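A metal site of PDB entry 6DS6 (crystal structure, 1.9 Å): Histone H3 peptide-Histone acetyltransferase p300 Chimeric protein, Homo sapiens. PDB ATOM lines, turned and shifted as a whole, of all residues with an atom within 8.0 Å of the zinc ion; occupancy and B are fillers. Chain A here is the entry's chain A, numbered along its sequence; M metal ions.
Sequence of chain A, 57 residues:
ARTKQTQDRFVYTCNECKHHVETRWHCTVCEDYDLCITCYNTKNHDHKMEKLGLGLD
The backbone NH of Cys 14 sits at hydrogen-bond distance from the backbone carbonyl oxygen of His 19.
SG of Cys 14 lies close to N of Glu 16.
A ring nitrogen (ND1) of His 19 sits at hydrogen-bond distance from the backbone carbonyl oxygen (O) of Cys 17, 2.7 Å away.
The zinc ion is bound by the side-chain sulfur (SG) of Cys 36 (2.1 Å), the side-chain sulfur (SG) of Cys 17 (2.3 Å), the side-chain sulfur (SG) of Cys 39 (2.4 Å) and the side-chain sulfur (SG) of Cys 14 (2.5 Å).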
ATOM      1  N   THR A  13       0.897 -30.798  -7.592  1.00  0.00           N
ATOM      2  CA  THR A  13       1.187 -29.378  -7.541  1.00  0.00           C
ATOM      3  C   THR A  13       1.182 -28.914  -6.085  1.00  0.00           C
ATOM      4  O   THR A  13       0.559 -29.542  -5.214  1.00  0.00           O
ATOM      5  CB  THR A  13       0.164 -28.541  -8.318  1.00  0.00           C
ATOM      6  OG1 THR A  13      -1.151 -28.824  -7.813  1.00  0.00           O
ATOM      7  CG2 THR A  13       0.218 -28.869  -9.818  1.00  0.00           C
ATOM      8  N   CYS A  14       1.884 -27.804  -5.819  1.00  0.00           N
ATOM      9  CA  CYS A  14       1.828 -27.198  -4.489  1.00  0.00           C
ATOM     10  C   CYS A  14       0.526 -26.439  -4.336  1.00  0.00           C
ATOM     11  O   CYS A  14       0.190 -25.594  -5.173  1.00  0.00           O
ATOM     12  CB  CYS A  14       3.011 -26.256  -4.262  1.00  0.00           C
ATOM     13  SG  CYS A  14       2.779 -25.231  -2.754  1.00  0.00           S
ATOM     14  N   ASN A  15      -0.224 -26.735  -3.272  1.00  0.00           N
ATOM     15  CA  ASN A  15      -1.505 -26.072  -3.103  1.00  0.00           C
ATOM     16  C   ASN A  15      -1.354 -24.560  -2.917  1.00  0.00           C
ATOM     17  O   ASN A  15      -2.319 -23.825  -3.138  1.00  0.00           O
ATOM     18  CB  ASN A  15      -2.258 -26.639  -1.899  1.00  0.00           C
ATOM     19  CG  ASN A  15      -2.877 -27.978  -2.168  1.00  0.00           C
ATOM     20  OD1 ASN A  15      -2.182 -28.961  -2.437  1.00  0.00           O
ATOM     21  ND2 ASN A  15      -4.194 -28.043  -2.045  1.00  0.00           N
ATOM     22  N   GLU A  16      -0.161 -24.092  -2.529  1.00  0.00           N
ATOM     23  CA  GLU A  16       0.088 -22.676  -2.262  1.00  0.00           C
ATOM     24  C   GLU A  16       0.540 -21.928  -3.514  1.00  0.00           C
ATOM     25  O   GLU A  16      -0.140 -21.001  -3.974  1.00  0.00           O
ATOM     26  CB  GLU A  16       1.114 -22.503  -1.143  1.00  0.00           C
ATOM     27  CG  GLU A  16       0.524 -22.696   0.221  1.00  0.00           C
ATOM     28  CD  GLU A  16      -0.686 -21.818   0.454  1.00  0.00           C
ATOM     29  OE1 GLU A  16      -0.545 -20.585   0.307  1.00  0.00           O
ATOM     30  OE2 GLU A  16      -1.766 -22.371   0.792  1.00  0.00           O
ATOM     31  N   CYS A  17       1.690 -22.294  -4.066  1.00  0.00           N
ATOM     32  CA  CYS A  17       2.211 -21.552  -5.216  1.00  0.00           C
ATOM     33  C   CYS A  17       1.763 -22.127  -6.555  1.00  0.00           C
ATOM     34  O   CYS A  17       2.093 -21.561  -7.590  1.00  0.00           O
ATOM     35  CB  CYS A  17       3.738 -21.462  -5.154  1.00  0.00           C
ATOM     36  SG  CYS A  17       4.698 -22.998  -5.284  1.00  0.00           S
ATOM     37  N   LYS A  18       1.010 -23.235  -6.550  1.00  0.00           N
ATOM     38  CA  LYS A  18       0.447 -23.886  -7.726  1.00  0.00           C
ATOM     39  C   LYS A  18       1.489 -24.468  -8.665  1.00  0.00           C
ATOM     40  O   LYS A  18       1.153 -24.926  -9.759  1.00  0.00           O
ATOM     41  CB  LYS A  18      -0.479 -22.960  -8.518  1.00  0.00           C
ATOM     42  CG  LYS A  18      -1.427 -22.123  -7.665  1.00  0.00           C
ATOM     43  CD  LYS A  18      -2.334 -22.985  -6.828  1.00  0.00           C
ATOM     44  CE  LYS A  18      -3.451 -22.176  -6.173  1.00  0.00           C
ATOM     45  NZ  LYS A  18      -4.376 -23.019  -5.367  1.00  0.00           N
ATOM     46  N   HIS A  19       2.767 -24.468  -8.267  1.00  0.00           N
ATOM     47  CA  HIS A  19       3.793 -25.052  -9.106  1.00  0.00           C
ATOM     48  C   HIS A  19       3.793 -26.575  -9.029  1.00  0.00           C
ATOM     49  O   HIS A  19       3.333 -27.170  -8.055  1.00  0.00           O
ATOM     50  CB  HIS A  19       5.181 -24.534  -8.710  1.00  0.00           C
ATOM     51  CG  HIS A  19       5.406 -23.098  -9.049  1.00  0.00           C
ATOM     52  ND1 HIS A  19       4.445 -22.119  -8.874  1.00  0.00           N
ATOM     53  CD2 HIS A  19       6.493 -22.458  -9.553  1.00  0.00           C
ATOM     54  CE1 HIS A  19       4.931 -20.951  -9.251  1.00  0.00           C
ATOM     55  NE2 HIS A  19       6.176 -21.134  -9.669  1.00  0.00           N
ATOM     56  N   HIS A  20       4.324 -27.184 -10.090  1.00  0.00           N
ATOM     57  CA  HIS A  20       4.586 -28.622 -10.134  1.00  0.00           C
ATOM     58  C   HIS A  20       5.605 -29.001  -9.063  1.00  0.00           C
ATOM     59  O   HIS A  20       6.628 -28.326  -8.898  1.00  0.00           O
ATOM     60  CB  HIS A  20       5.091 -28.998 -11.536  1.00  0.00           C
ATOM     61  CG  HIS A  20       5.526 -30.436 -11.686  1.00  0.00           C
ATOM     62  ND1 HIS A  20       4.642 -31.497 -11.690  1.00  0.00           N
ATOM     63  CD2 HIS A  20       6.755 -30.971 -11.893  1.00  0.00           C
ATOM     64  CE1 HIS A  20       5.304 -32.625 -11.863  1.00  0.00           C
ATOM     65  NE2 HIS A  20       6.592 -32.336 -11.988  1.00  0.00           N
ATOM     66  N   VAL A  21       5.329 -30.086  -8.340  1.00  0.00           N
ATOM     67  CA  VAL A  21       6.236 -30.584  -7.306  1.00  0.00           C
ATOM     68  C   VAL A  21       6.444 -32.074  -7.507  1.00  0.00           C
ATOM     69  O   VAL A  21       5.510 -32.793  -7.871  1.00  0.00           O
ATOM     70  CB  VAL A  21       5.712 -30.308  -5.880  1.00  0.00           C
ATOM     71  CG1 VAL A  21       5.888 -28.853  -5.556  1.00  0.00           C
ATOM     72  CG2 VAL A  21       4.232 -30.686  -5.741  1.00  0.00           C
ATOM     73  N   ASP A  34      -0.725 -30.523  -0.621  1.00  0.00           N
ATOM     74  CA  ASP A  34       0.715 -30.679  -0.726  1.00  0.00           C
ATOM     75  C   ASP A  34       1.382 -29.303  -0.764  1.00  0.00           C
ATOM     76  O   ASP A  34       0.802 -28.331  -1.245  1.00  0.00           O
ATOM     77  CB  ASP A  34       1.094 -31.499  -1.973  1.00  0.00           C
ATOM     78  CG  ASP A  34       0.454 -32.868  -1.986  1.00  0.00           C
ATOM     79  OD1 ASP A  34       1.026 -33.799  -1.391  1.00  0.00           O
ATOM     80  OD2 ASP A  34      -0.659 -33.019  -2.565  1.00  0.00           O
ATOM     81  N   LEU A  35       2.623 -29.239  -0.277  1.00  0.00           N
ATOM     82  CA  LEU A  35       3.438 -28.039  -0.348  1.00  0.00           C
ATOM     83  C   LEU A  35       4.792 -28.363  -0.949  1.00  0.00           C
ATOM     84  O   LEU A  35       5.403 -29.389  -0.623  1.00  0.00           O
ATOM     85  CB  LEU A  35       3.663 -27.414   1.045  1.00  0.00           C
ATOM     86  CG  LEU A  35       2.458 -26.845   1.784  1.00  0.00           C
ATOM     87  CD1 LEU A  35       2.904 -26.265   3.116  1.00  0.00           C
ATOM     88  CD2 LEU A  35       1.818 -25.772   0.919  1.00  0.00           C
ATOM     89  N   CYS A  36       5.279 -27.466  -1.803  1.00  0.00           N
ATOM     90  CA  CYS A  36       6.682 -27.477  -2.170  1.00  0.00           C
ATOM     91  C   CYS A  36       7.539 -27.154  -0.956  1.00  0.00           C
ATOM     92  O   CYS A  36       7.062 -26.654   0.066  1.00  0.00           O
ATOM     93  CB  CYS A  36       6.960 -26.496  -3.320  1.00  0.00           C
ATOM     94  SG  CYS A  36       6.775 -24.718  -2.932  1.00  0.00           S
ATOM     95  N   ILE A  37       8.835 -27.456  -1.073  1.00  0.00           N
ATOM     96  CA  ILE A  37       9.715 -27.280   0.074  1.00  0.00           C
ATOM     97  C   ILE A  37       9.786 -25.815   0.482  1.00  0.00           C
ATOM     98  O   ILE A  37       9.757 -25.480   1.672  1.00  0.00           O
ATOM     99  CB  ILE A  37      11.100 -27.860  -0.239  1.00  0.00           C
ATOM    100  CG1 ILE A  37      10.981 -29.377  -0.423  1.00  0.00           C
ATOM    101  CG2 ILE A  37      12.081 -27.514   0.872  1.00  0.00           C
ATOM    102  CD1 ILE A  37      12.230 -30.130  -0.103  1.00  0.00           C
ATOM    103  N   THR A  38       9.832 -24.901  -0.494  1.00  0.00           N
ATOM    104  CA  THR A  38       9.905 -23.488  -0.170  1.00  0.00           C
ATOM    105  C   THR A  38       8.671 -23.024   0.580  1.00  0.00           C
ATOM    106  O   THR A  38       8.774 -22.364   1.622  1.00  0.00           O
ATOM    107  CB  THR A  38      10.117 -22.678  -1.442  1.00  0.00           C
ATOM    108  OG1 THR A  38      11.139 -23.308  -2.236  1.00  0.00           O
ATOM    109  CG2 THR A  38      10.553 -21.279  -1.098  1.00  0.00           C
ATOM    110  N   CYS A  39       7.488 -23.372   0.085  1.00  0.00           N
ATOM    111  CA  CYS A  39       6.259 -22.998   0.785  1.00  0.00           C
ATOM    112  C   CYS A  39       6.112 -23.698   2.139  1.00  0.00           C
ATOM    113  O   CYS A  39       5.551 -23.114   3.067  1.00  0.00           O
ATOM    114  CB  CYS A  39       5.040 -23.319  -0.088  1.00  0.00           C
ATOM    115  SG  CYS A  39       4.776 -22.183  -1.462  1.00  0.00           S
ATOM    116  N   TYR A  40       6.603 -24.941   2.264  1.00  0.00           N
ATOM    117  CA  TYR A  40       6.599 -25.603   3.569  1.00  0.00           C
ATOM    118  C   TYR A  40       7.382 -24.775   4.574  1.00  0.00           C
ATOM    119  O   TYR A  40       6.908 -24.507   5.686  1.00  0.00           O
ATOM    120  CB  TYR A  40       7.206 -27.009   3.494  1.00  0.00           C
ATOM    121  CG  TYR A  40       7.274 -27.657   4.876  1.00  0.00           C
ATOM    122  CD1 TYR A  40       6.147 -28.192   5.448  1.00  0.00           C
ATOM    123  CD2 TYR A  40       8.450 -27.680   5.629  1.00  0.00           C
ATOM    124  CE1 TYR A  40       6.174 -28.758   6.722  1.00  0.00           C
ATOM    125  CE2 TYR A  40       8.475 -28.236   6.924  1.00  0.00           C
ATOM    126  CZ  TYR A  40       7.317 -28.780   7.460  1.00  0.00           C
ATOM    127  OH  TYR A  40       7.250 -29.349   8.720  1.00  0.00           O
ATOM    128  N   THR A  42       7.968 -21.713   4.503  1.00  0.00           N
ATOM    129  CA  THR A  42       7.543 -20.326   4.518  1.00  0.00           C
ATOM    130  C   THR A  42       6.198 -20.124   5.183  1.00  0.00           C
ATOM    131  O   THR A  42       6.070 -19.284   6.085  1.00  0.00           O
ATOM    132  CB  THR A  42       7.501 -19.770   3.080  1.00  0.00           C
ATOM    133  OG1 THR A  42       8.835 -19.437   2.653  1.00  0.00           O
ATOM    134  CG2 THR A  42       6.632 -18.519   3.008  1.00  0.00           C
HETATM  135 ZN    ZN M   1       4.857 -23.921  -3.150  1.00  0.00          ZN
